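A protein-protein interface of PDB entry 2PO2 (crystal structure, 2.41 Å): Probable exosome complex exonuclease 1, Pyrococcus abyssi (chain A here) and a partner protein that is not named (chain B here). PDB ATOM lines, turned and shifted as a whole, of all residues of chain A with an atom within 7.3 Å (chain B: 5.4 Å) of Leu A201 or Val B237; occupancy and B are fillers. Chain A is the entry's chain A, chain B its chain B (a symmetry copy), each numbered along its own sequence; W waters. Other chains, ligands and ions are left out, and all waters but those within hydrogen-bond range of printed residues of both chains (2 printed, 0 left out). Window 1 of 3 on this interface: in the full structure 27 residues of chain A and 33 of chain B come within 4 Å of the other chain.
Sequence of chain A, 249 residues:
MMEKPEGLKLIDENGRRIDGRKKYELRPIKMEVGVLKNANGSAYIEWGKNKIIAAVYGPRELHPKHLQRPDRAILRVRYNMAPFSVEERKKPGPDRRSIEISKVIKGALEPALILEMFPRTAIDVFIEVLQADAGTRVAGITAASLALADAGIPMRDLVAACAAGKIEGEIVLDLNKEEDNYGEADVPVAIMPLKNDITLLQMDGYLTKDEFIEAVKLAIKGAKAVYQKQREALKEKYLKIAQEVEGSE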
ATOM      1  N   GLU A 100     -18.688 -21.894  23.174  1.00  0.00           N
ATOM      2  CA  GLU A 100     -18.894 -21.859  21.736  1.00  0.00           C
ATOM      3  C   GLU A 100     -18.502 -20.507  21.200  1.00  0.00           C
ATOM      4  O   GLU A 100     -17.911 -20.428  20.154  1.00  0.00           O
ATOM      5  CB  GLU A 100     -20.329 -22.201  21.338  1.00  0.00           C
ATOM      6  CG  GLU A 100     -20.618 -21.960  19.835  1.00  0.00           C
ATOM      7  CD  GLU A 100     -22.088 -21.793  19.513  1.00  0.00           C
ATOM      8  OE1 GLU A 100     -22.948 -21.747  20.411  1.00  0.00           O
ATOM      9  OE2 GLU A 100     -22.402 -21.688  18.321  1.00  0.00           O
ATOM     10  N   VAL A 104     -15.656 -19.760  18.234  1.00  0.00           N
ATOM     11  CA  VAL A 104     -16.141 -19.134  17.042  1.00  0.00           C
ATOM     12  C   VAL A 104     -15.437 -17.760  16.810  1.00  0.00           C
ATOM     13  O   VAL A 104     -15.164 -17.375  15.648  1.00  0.00           O
ATOM     14  CB  VAL A 104     -17.737 -19.182  17.171  1.00  0.00           C
ATOM     15  CG1 VAL A 104     -18.426 -17.768  17.301  1.00  0.00           C
ATOM     16  CG2 VAL A 104     -18.347 -20.105  16.129  1.00  0.00           C
ATOM     17  N   ALA A 108     -12.444 -16.902  13.857  1.00  0.00           N
ATOM     18  CA  ALA A 108     -12.642 -15.609  13.194  1.00  0.00           C
ATOM     19  C   ALA A 108     -11.371 -14.818  13.137  1.00  0.00           C
ATOM     20  O   ALA A 108     -11.176 -14.017  12.183  1.00  0.00           O
ATOM     21  CB  ALA A 108     -13.702 -14.774  13.920  1.00  0.00           C
ATOM     22  N   ASP A 186     -30.625 -14.019  14.442  1.00  0.00           N
ATOM     23  CA  ASP A 186     -29.430 -13.312  14.802  1.00  0.00           C
ATOM     24  C   ASP A 186     -28.411 -13.818  13.807  1.00  0.00           C
ATOM     25  O   ASP A 186     -28.220 -15.026  13.696  1.00  0.00           O
ATOM     26  CB  ASP A 186     -28.964 -13.725  16.199  1.00  0.00           C
ATOM     27  CG  ASP A 186     -27.835 -12.833  16.745  1.00  0.00           C
ATOM     28  OD1 ASP A 186     -27.421 -13.081  17.910  1.00  0.00           O
ATOM     29  OD2 ASP A 186     -27.381 -11.879  16.044  1.00  0.00           O
ATOM     30  N   VAL A 187     -27.792 -12.903  13.065  1.00  0.00           N
ATOM     31  CA  VAL A 187     -26.792 -13.267  12.065  1.00  0.00           C
ATOM     32  C   VAL A 187     -25.529 -12.441  12.259  1.00  0.00           C
ATOM     33  O   VAL A 187     -25.407 -11.383  11.632  1.00  0.00           O
ATOM     34  CB  VAL A 187     -27.316 -13.139  10.612  1.00  0.00           C
ATOM     35  CG1 VAL A 187     -26.372 -13.787   9.668  1.00  0.00           C
ATOM     36  CG2 VAL A 187     -28.648 -13.828  10.494  1.00  0.00           C
ATOM     37  N   PRO A 188     -24.624 -12.891  13.164  1.00  0.00           N
ATOM     38  CA  PRO A 188     -23.323 -12.295  13.318  1.00  0.00           C
ATOM     39  C   PRO A 188     -22.460 -12.733  12.144  1.00  0.00           C
ATOM     40  O   PRO A 188     -22.564 -13.879  11.679  1.00  0.00           O
ATOM     41  CB  PRO A 188     -22.785 -12.922  14.626  1.00  0.00           C
ATOM     42  CG  PRO A 188     -23.478 -14.124  14.800  1.00  0.00           C
ATOM     43  CD  PRO A 188     -24.804 -14.014  14.107  1.00  0.00           C
ATOM     44  N   VAL A 189     -21.633 -11.796  11.674  1.00  0.00           N
ATOM     45  CA  VAL A 189     -20.716 -12.025  10.582  1.00  0.00           C
ATOM     46  C   VAL A 189     -19.405 -11.352  10.992  1.00  0.00           C
ATOM     47  O   VAL A 189     -19.388 -10.224  11.476  1.00  0.00           O
ATOM     48  CB  VAL A 189     -21.265 -11.406   9.271  1.00  0.00           C
ATOM     49  CG1 VAL A 189     -20.298 -11.597   8.115  1.00  0.00           C
ATOM     50  CG2 VAL A 189     -22.581 -12.032   8.918  1.00  0.00           C
ATOM     51  N   ALA A 190     -18.290 -12.038  10.802  1.00  0.00           N
ATOM     52  CA  ALA A 190     -17.004 -11.373  10.930  1.00  0.00           C
ATOM     53  C   ALA A 190     -16.361 -11.598   9.609  1.00  0.00           C
ATOM     54  O   ALA A 190     -16.469 -12.684   9.038  1.00  0.00           O
ATOM     55  CB  ALA A 190     -16.175 -11.967  12.086  1.00  0.00           C
ATOM     56  N   ILE A 198     -15.152 -13.952   4.878  1.00  0.00           N
ATOM     57  CA  ILE A 198     -15.989 -14.083   6.034  1.00  0.00           C
ATOM     58  C   ILE A 198     -15.351 -15.126   6.949  1.00  0.00           C
ATOM     59  O   ILE A 198     -15.206 -16.292   6.564  1.00  0.00           O
ATOM     60  CB  ILE A 198     -17.404 -14.536   5.653  1.00  0.00           C
ATOM     61  CG1 ILE A 198     -18.069 -13.543   4.690  1.00  0.00           C
ATOM     62  CG2 ILE A 198     -18.232 -14.862   6.908  1.00  0.00           C
ATOM     63  CD1 ILE A 198     -19.050 -14.196   3.781  1.00  0.00           C
ATOM     64  N   THR A 199     -14.964 -14.699   8.159  1.00  0.00           N
ATOM     65  CA  THR A 199     -14.267 -15.573   9.064  1.00  0.00           C
ATOM     66  C   THR A 199     -15.121 -16.055  10.225  1.00  0.00           C
ATOM     67  O   THR A 199     -14.704 -16.926  10.979  1.00  0.00           O
ATOM     68  CB  THR A 199     -12.949 -14.943   9.567  1.00  0.00           C
ATOM     69  OG1 THR A 199     -13.209 -13.776  10.388  1.00  0.00           O
ATOM     70  CG2 THR A 199     -12.043 -14.615   8.384  1.00  0.00           C
ATOM     71  N   LEU A 200     -16.303 -15.462  10.367  1.00  0.00           N
ATOM     72  CA  LEU A 200     -17.355 -15.880  11.278  1.00  0.00           C
ATOM     73  C   LEU A 200     -18.665 -15.695  10.561  1.00  0.00           C
ATOM     74  O   LEU A 200     -18.923 -14.663   9.938  1.00  0.00           O
ATOM     75  CB  LEU A 200     -17.370 -15.058  12.575  1.00  0.00           C
ATOM     76  CG  LEU A 200     -18.483 -15.454  13.568  1.00  0.00           C
ATOM     77  CD1 LEU A 200     -17.928 -15.796  14.901  1.00  0.00           C
ATOM     78  CD2 LEU A 200     -19.635 -14.489  13.741  1.00  0.00           C
ATOM     79  N   LEU A 201     -19.498 -16.712  10.635  1.00  0.00           N
ATOM     80  CA  LEU A 201     -20.838 -16.616  10.093  1.00  0.00           C
ATOM     81  C   LEU A 201     -21.733 -17.522  10.901  1.00  0.00           C
ATOM     82  O   LEU A 201     -21.569 -18.723  10.871  1.00  0.00           O
ATOM     83  CB  LEU A 201     -20.879 -16.967   8.589  1.00  0.00           C
ATOM     84  CG  LEU A 201     -21.895 -16.187   7.762  1.00  0.00           C
ATOM     85  CD1 LEU A 201     -22.163 -16.776   6.373  1.00  0.00           C
ATOM     86  CD2 LEU A 201     -23.177 -16.054   8.493  1.00  0.00           C
ATOM     87  N   GLN A 202     -22.708 -16.944  11.595  1.00  0.00           N
ATOM     88  CA  GLN A 202     -23.620 -17.760  12.379  1.00  0.00           C
ATOM     89  C   GLN A 202     -25.030 -17.299  12.174  1.00  0.00           C
ATOM     90  O   GLN A 202     -25.283 -16.115  11.938  1.00  0.00           O
ATOM     91  CB  GLN A 202     -23.276 -17.708  13.873  1.00  0.00           C
ATOM     92  CG  GLN A 202     -21.906 -18.208  14.169  1.00  0.00           C
ATOM     93  CD  GLN A 202     -21.646 -18.167  15.606  1.00  0.00           C
ATOM     94  OE1 GLN A 202     -21.305 -17.095  16.167  1.00  0.00           O
ATOM     95  NE2 GLN A 202     -21.823 -19.329  16.268  1.00  0.00           N
ATOM     96  N   MET A 203     -25.954 -18.247  12.263  1.00  0.00           N
ATOM     97  CA  MET A 203     -27.348 -17.905  12.102  1.00  0.00           C
ATOM     98  C   MET A 203     -28.093 -18.700  13.117  1.00  0.00           C
ATOM     99  O   MET A 203     -28.005 -19.918  13.197  1.00  0.00           O
ATOM    100  CB  MET A 203     -27.869 -18.147  10.662  1.00  0.00           C
ATOM    101  CG  MET A 203     -29.199 -17.503  10.369  1.00  0.00           C
ATOM    102  SD  MET A 203     -30.569 -18.311  11.196  1.00  0.00           S
ATOM    103  CE  MET A 203     -30.865 -19.680  10.149  1.00  0.00           C
ATOM    104  N   ASP A 204     -28.842 -17.959  13.896  1.00  0.00           N
ATOM    105  CA  ASP A 204     -29.607 -18.480  14.978  1.00  0.00           C
ATOM    106  C   ASP A 204     -30.965 -17.941  14.699  1.00  0.00           C
ATOM    107  O   ASP A 204     -31.098 -16.748  14.432  1.00  0.00           O
ATOM    108  CB  ASP A 204     -29.102 -17.791  16.218  1.00  0.00           C
ATOM    109  CG  ASP A 204     -29.600 -18.402  17.391  1.00  0.00           C
ATOM    110  OD1 ASP A 204     -30.392 -19.329  17.200  1.00  0.00           O
ATOM    111  OD2 ASP A 204     -29.207 -18.006  18.506  1.00  0.00           O
ATOM    112  N   GLY A 205     -31.991 -18.766  14.746  1.00  0.00           N
ATOM    113  CA  GLY A 205     -33.256 -18.282  14.275  1.00  0.00           C
ATOM    114  C   GLY A 205     -33.777 -19.058  13.079  1.00  0.00           C
ATOM    115  O   GLY A 205     -33.588 -20.275  12.994  1.00  0.00           O
ATOM    116  N   PHE A 212     -31.620 -14.894   4.681  1.00  0.00           N
ATOM    117  CA  PHE A 212     -30.330 -15.157   5.272  1.00  0.00           C
ATOM    118  C   PHE A 212     -29.230 -14.395   4.521  1.00  0.00           C
ATOM    119  O   PHE A 212     -28.473 -13.660   5.123  1.00  0.00           O
ATOM    120  CB  PHE A 212     -30.041 -16.667   5.353  1.00  0.00           C
ATOM    121  CG  PHE A 212     -28.599 -16.982   5.698  1.00  0.00           C
ATOM    122  CD1 PHE A 212     -27.784 -17.639   4.791  1.00  0.00           C
ATOM    123  CD2 PHE A 212     -28.052 -16.555   6.901  1.00  0.00           C
ATOM    124  CE1 PHE A 212     -26.471 -17.897   5.107  1.00  0.00           C
ATOM    125  CE2 PHE A 212     -26.753 -16.804   7.206  1.00  0.00           C
ATOM    126  CZ  PHE A 212     -25.962 -17.472   6.322  1.00  0.00           C
ATOM    127  N   ILE A 213     -29.150 -14.570   3.205  1.00  0.00           N
ATOM    128  CA  ILE A 213     -28.183 -13.835   2.378  1.00  0.00           C
ATOM    129  C   ILE A 213     -28.276 -12.299   2.569  1.00  0.00           C
ATOM    130  O   ILE A 213     -27.259 -11.604   2.644  1.00  0.00           O
ATOM    131  CB  ILE A 213     -28.258 -14.252   0.843  1.00  0.00           C
ATOM    132  CG1 ILE A 213     -27.950 -15.747   0.636  1.00  0.00           C
ATOM    133  CG2 ILE A 213     -27.347 -13.399  -0.012  1.00  0.00           C
ATOM    134  CD1 ILE A 213     -26.722 -16.264   1.445  1.00  0.00           C
ATOM    135  N   ALA A 215     -29.334 -10.663   5.189  1.00  0.00           N
ATOM    136  CA  ALA A 215     -28.813 -10.397   6.538  1.00  0.00           C
ATOM    137  C   ALA A 215     -27.291 -10.544   6.557  1.00  0.00           C
ATOM    138  O   ALA A 215     -26.590  -9.708   7.128  1.00  0.00           O
ATOM    139  CB  ALA A 215     -29.485 -11.278   7.577  1.00  0.00           C
ATOM    140  N   VAL A 216     -26.767 -11.568   5.884  1.00  0.00           N
ATOM    141  CA  VAL A 216     -25.314 -11.700   5.741  1.00  0.00           C
ATOM    142  C   VAL A 216     -24.686 -10.515   5.026  1.00  0.00           C
ATOM    143  O   VAL A 216     -23.631 -10.069   5.425  1.00  0.00           O
ATOM    144  CB  VAL A 216     -24.888 -13.068   5.151  1.00  0.00           C
ATOM    145  CG1 VAL A 216     -23.418 -13.076   4.753  1.00  0.00           C
ATOM    146  CG2 VAL A 216     -25.137 -14.139   6.178  1.00  0.00           C
ATOM    147  N   ILE A 220     -22.385  -7.510   6.777  1.00  0.00           N
ATOM    148  CA  ILE A 220     -21.103  -7.177   6.197  1.00  0.00           C
ATOM    149  C   ILE A 220     -21.059  -5.662   5.909  1.00  0.00           C
ATOM    150  O   ILE A 220     -20.049  -5.037   6.166  1.00  0.00           O
ATOM    151  CB  ILE A 220     -20.730  -8.026   4.924  1.00  0.00           C
ATOM    152  CG1 ILE A 220     -20.705  -9.541   5.214  1.00  0.00           C
ATOM    153  CG2 ILE A 220     -19.418  -7.585   4.352  1.00  0.00           C
ATOM    154  CD1 ILE A 220     -20.835 -10.386   3.928  1.00  0.00           C
ATOM    155  N   ARG B 115     -29.903 -25.785  18.055  1.00  0.00           N
ATOM    156  CA  ARG B 115     -30.446 -24.576  17.454  1.00  0.00           C
ATOM    157  C   ARG B 115     -31.190 -24.989  16.214  1.00  0.00           C
ATOM    158  O   ARG B 115     -32.266 -24.443  15.911  1.00  0.00           O
ATOM    159  CB  ARG B 115     -29.338 -23.600  17.053  1.00  0.00           C
ATOM    160  CG  ARG B 115     -28.677 -23.019  18.264  1.00  0.00           C
ATOM    161  CD  ARG B 115     -28.006 -21.699  18.039  1.00  0.00           C
ATOM    162  NE  ARG B 115     -27.115 -21.707  16.905  1.00  0.00           N
ATOM    163  CZ  ARG B 115     -25.797 -21.903  17.012  1.00  0.00           C
ATOM    164  NH1 ARG B 115     -25.011 -21.838  15.913  1.00  0.00           N
ATOM    165  NH2 ARG B 115     -25.289 -22.138  18.213  1.00  0.00           N
ATOM    166  N   ILE B 224     -18.406 -24.990   7.070  1.00  0.00           N
ATOM    167  CA  ILE B 224     -19.638 -24.243   7.194  1.00  0.00           C
ATOM    168  C   ILE B 224     -20.711 -25.262   7.136  1.00  0.00           C
ATOM    169  O   ILE B 224     -20.619 -26.200   6.354  1.00  0.00           O
ATOM    170  CB  ILE B 224     -19.839 -23.117   6.094  1.00  0.00           C
ATOM    171  CG1 ILE B 224     -20.955 -22.147   6.518  1.00  0.00           C
ATOM    172  CG2 ILE B 224     -20.078 -23.689   4.711  1.00  0.00           C
ATOM    173  CD1 ILE B 224     -21.107 -20.940   5.509  1.00  0.00           C
ATOM    174  N   THR B 225     -21.692 -25.069   7.997  1.00  0.00           N
ATOM    175  CA  THR B 225     -22.815 -25.963   8.185  1.00  0.00           C
ATOM    176  C   THR B 225     -24.046 -25.138   8.006  1.00  0.00           C
ATOM    177  O   THR B 225     -24.187 -24.072   8.609  1.00  0.00           O
ATOM    178  CB  THR B 225     -22.796 -26.566   9.630  1.00  0.00           C
ATOM    179  OG1 THR B 225     -21.652 -27.446   9.780  1.00  0.00           O
ATOM    180  CG2 THR B 225     -24.080 -27.259   9.946  1.00  0.00           C
ATOM    181  N   ILE B 226     -24.903 -25.609   7.104  1.00  0.00           N
ATOM    182  CA  ILE B 226     -26.241 -25.023   6.840  1.00  0.00           C
ATOM    183  C   ILE B 226     -27.282 -26.048   7.174  1.00  0.00           C
ATOM    184  O   ILE B 226     -27.255 -27.161   6.677  1.00  0.00           O
ATOM    185  CB  ILE B 226     -26.476 -24.528   5.358  1.00  0.00           C
ATOM    186  CG1 ILE B 226     -25.198 -23.899   4.793  1.00  0.00           C
ATOM    187  CG2 ILE B 226     -27.623 -23.527   5.298  1.00  0.00           C
ATOM    188  CD1 ILE B 226     -24.766 -22.691   5.551  1.00  0.00           C
ATOM    189  N   THR B 227     -28.199 -25.647   8.026  1.00  0.00           N
ATOM    190  CA  THR B 227     -29.217 -26.530   8.509  1.00  0.00           C
ATOM    191  C   THR B 227     -30.522 -26.041   8.001  1.00  0.00           C
ATOM    192  O   THR B 227     -30.873 -24.906   8.214  1.00  0.00           O
ATOM    193  CB  THR B 227     -29.202 -26.591  10.080  1.00  0.00           C
ATOM    194  OG1 THR B 227     -28.073 -27.363  10.468  1.00  0.00           O
ATOM    195  CG2 THR B 227     -30.488 -27.255  10.645  1.00  0.00           C
ATOM    196  N   ILE B 234     -33.883 -22.011   6.840  1.00  0.00           N
ATOM    197  CA  ILE B 234     -32.600 -22.360   7.405  1.00  0.00           C
ATOM    198  C   ILE B 234     -32.842 -22.097   8.840  1.00  0.00           C
ATOM    199  O   ILE B 234     -33.291 -21.000   9.167  1.00  0.00           O
ATOM    200  CB  ILE B 234     -31.462 -21.383   6.932  1.00  0.00           C
ATOM    201  CG1 ILE B 234     -31.470 -21.185   5.421  1.00  0.00           C
ATOM    202  CG2 ILE B 234     -30.123 -21.818   7.437  1.00  0.00           C
ATOM    203  CD1 ILE B 234     -30.615 -20.040   5.006  1.00  0.00           C
ATOM    204  N   SER B 235     -32.595 -23.085   9.694  1.00  0.00           N
ATOM    205  CA  SER B 235     -32.658 -22.892  11.158  1.00  0.00           C
ATOM    206  C   SER B 235     -31.327 -22.759  11.837  1.00  0.00           C
ATOM    207  O   SER B 235     -31.321 -22.479  13.039  1.00  0.00           O
ATOM    208  CB  SER B 235     -33.456 -23.999  11.861  1.00  0.00           C
ATOM    209  OG  SER B 235     -33.058 -25.299  11.466  1.00  0.00           O
ATOM    210  N   ALA B 236     -30.207 -22.957  11.108  1.00  0.00           N
ATOM    211  CA  ALA B 236     -28.839 -22.717  11.640  1.00  0.00           C
ATOM    212  C   ALA B 236     -27.830 -22.682  10.552  1.00  0.00           C
ATOM    213  O   ALA B 236     -27.897 -23.436   9.581  1.00  0.00           O
ATOM    214  CB  ALA B 236     -28.386 -23.796  12.644  1.00  0.00           C
ATOM    215  N   VAL B 237     -26.855 -21.817  10.787  1.00  0.00           N
ATOM    216  CA  VAL B 237     -25.642 -21.731  10.027  1.00  0.00           C
ATOM    217  C   VAL B 237     -24.559 -21.625  11.064  1.00  0.00           C
ATOM    218  O   VAL B 237     -24.656 -20.860  12.039  1.00  0.00           O
ATOM    219  CB  VAL B 237     -25.616 -20.434   9.107  1.00  0.00           C
ATOM    220  CG1 VAL B 237     -24.259 -20.309   8.365  1.00  0.00           C
ATOM    221  CG2 VAL B 237     -26.795 -20.442   8.144  1.00  0.00           C
ATOM    222  N   GLN B 238     -23.523 -22.409  10.850  1.00  0.00           N
ATOM    223  CA  GLN B 238     -22.330 -22.331  11.613  1.00  0.00           C
ATOM    224  C   GLN B 238     -21.084 -22.558  10.735  1.00  0.00           C
ATOM    225  O   GLN B 238     -20.756 -23.675  10.319  1.00  0.00           O
ATOM    226  CB  GLN B 238     -22.377 -23.346  12.755  1.00  0.00           C
ATOM    227  CG  GLN B 238     -21.206 -23.222  13.669  1.00  0.00           C
ATOM    228  CD  GLN B 238     -21.462 -22.450  14.961  1.00  0.00           C
ATOM    229  OE1 GLN B 238     -22.248 -21.546  15.014  1.00  0.00           O
ATOM    230  NE2 GLN B 238     -20.749 -22.850  16.043  1.00  0.00           N
ATOM    231  N   LYS B 239     -20.381 -21.475  10.494  1.00  0.00           N
ATOM    232  CA  LYS B 239     -19.005 -21.540  10.107  1.00  0.00           C
ATOM    233  C   LYS B 239     -18.266 -21.884  11.388  1.00  0.00           C
ATOM    234  O   LYS B 239     -18.438 -21.195  12.435  1.00  0.00           O
ATOM    235  CB  LYS B 239     -18.541 -20.218   9.560  1.00  0.00           C
ATOM    236  CG  LYS B 239     -17.211 -20.296   8.886  1.00  0.00           C
ATOM    237  CD  LYS B 239     -16.099 -19.832   9.798  1.00  0.00           C
ATOM    238  CE  LYS B 239     -14.744 -19.979   9.160  1.00  0.00           C
ATOM    239  NZ  LYS B 239     -13.756 -19.353  10.058  1.00  0.00           N
ATOM    240  N   VAL B 250     -20.884 -19.140   0.627  1.00  0.00           N
ATOM    241  CA  VAL B 250     -22.044 -19.241   1.492  1.00  0.00           C
ATOM    242  C   VAL B 250     -23.332 -19.466   0.672  1.00  0.00           C
ATOM    243  O   VAL B 250     -24.026 -20.450   0.851  1.00  0.00           O
ATOM    244  CB  VAL B 250     -22.119 -17.991   2.425  1.00  0.00           C
ATOM    245  CG1 VAL B 250     -23.385 -18.029   3.295  1.00  0.00           C
ATOM    246  CG2 VAL B 250     -20.876 -17.955   3.258  1.00  0.00           C
HETATM  247  O   HOH W   1     -18.589 -18.668  12.780  1.00  0.00           O
HETATM  248  O   HOH W   2     -23.931 -19.261  18.554  1.00  0.00           O
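Water W1 lies within hydrogen-bond range of O of Lys B239 (2.6 Å) and N of Leu A201 (3.0 Å). Water W2 lies within hydrogen-bond range of the side-chain carboxylate of Glu A100 (2.9 Å), the side-chain amide nitrogen of Gln A202 (3.1 Å) and the guanidinium group of Arg B115 (3.2 Å).
Among the printed residues, pairs that only touch across the chains: Met A203 with Ile B234 (2.9 Å), Gln A202 with Val B237 (3.3 Å), Met A203 with Ala B236 (3.3 Å), Phe A212 with Ile B234 (3.4 Å), Asp A204 with Arg B115 (3.5 Å), Leu A201 with Val B250 (3.5 Å), Met A203 with Ser B235 (3.5 Å), Phe A212 with Val B250 (3.6 Å), Phe A212 with Val B237 (3.6 Å), Val A104 with Gln B238 (3.6 Å), Leu A201 with Gln B238 (3.8 Å), Val A104 with Lys B239 (3.9 Å), Gly A205 with Ile B234 (3.9 Å) and Leu A201 with Val B237 (3.9 Å).
The backbone carbonyl oxygen (O) of Leu A201 sits at hydrogen-bond distance from the backbone NH (N) of Lys B239 (3.0 Å). The backbone NH of Met A203 sits at hydrogen-bond distance from the backbone carbonyl oxygen of Val B237 (2.9 Å). The backbone carbonyl oxygen (O) of Thr A199 lies within hydrogen-bond range of the side-chain amino group (NZ) of Lys B239, 2.8 Å away. The side-chain amide nitrogen of Gln A202 lies within hydrogen-bond range of the side-chain amide oxygen of Gln B238. The backbone carbonyl oxygen (O) of Gly A205 lies close to the backbone carbonyl oxygen (O) of Ser B235 (3.2 Å). The side-chain carboxylate of Glu A100 sits at hydrogen-bond distance from the side-chain amide nitrogen of Gln B238, at 3.0 Å. The guanidinium group (NH2) of Arg B115 lies within salt-bridge range of the side-chain carboxylate (OE2) of Glu A100 (2.9 Å).
N of Thr B227 lies within hydrogen-bond range of O of Ala B236 (2.7 Å). The guanidinium group (NH1) of Arg B115 is in hydrogen-bond range of the side-chain amide oxygen (OE1) of Gln B238 (2.9 Å). The backbone NH (N) of Ser B235 is in hydrogen-bond range of the backbone carbonyl oxygen (O) of Thr B227, 2.9 Å away. The side-chain hydroxyl (OG1) of Thr A199 lies within hydrogen-bond range of the backbone carbonyl oxygen (O) of Ala A108, 2.7 Å away. The backbone NH (N) of Asp A186 lies within hydrogen-bond range of the backbone carbonyl oxygen (O) of Asp A204. O of Ala A190 sits at hydrogen-bond distance from N of Thr A199, at 2.7 Å.
Val B237 touches four residues of chain A. Of the printed residues of chain A, Lys B239 touches Val A104 (3.9 Å), Thr A199 (2.8 Å) and Leu A201 (3.0 Å). Of the printed residues of chain A, Gln B238 touches Glu A100, Val A104, Leu A201 and Gln A202. Of the printed residues of chain B, Thr A199 touches Lys B239. Of the printed residues of chain B, Asp A204 touches Arg B115. The nearest residue of chain B that does not touch Leu A201 is Ile B224 (4.4 Å). The nearest residue of chain A that does not touch Val B237 is Asp A204 (5.3 Å). The nearest printed residue of chain A that does not touch Lys B239 is Leu A200 (4.4 Å).
Of the 12 printed residues of chain B, 8 touch a printed residue of chain A. Printed residues of chain B that touch a printed residue of chain A: Arg B115, Ile B234, Ser B235, Ala B236, Val B237, Gln B238, Lys B239 and Val B250. Hydrophobic or aromatic side chains of chain B that line the printed part of chain A: Ile B234, Ala B236, Val B237 and Val B250. Hydrophobic or aromatic side chains of chain A that line the printed part of chain B: Val A104, Leu A201, Met A203 and Phe A212.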
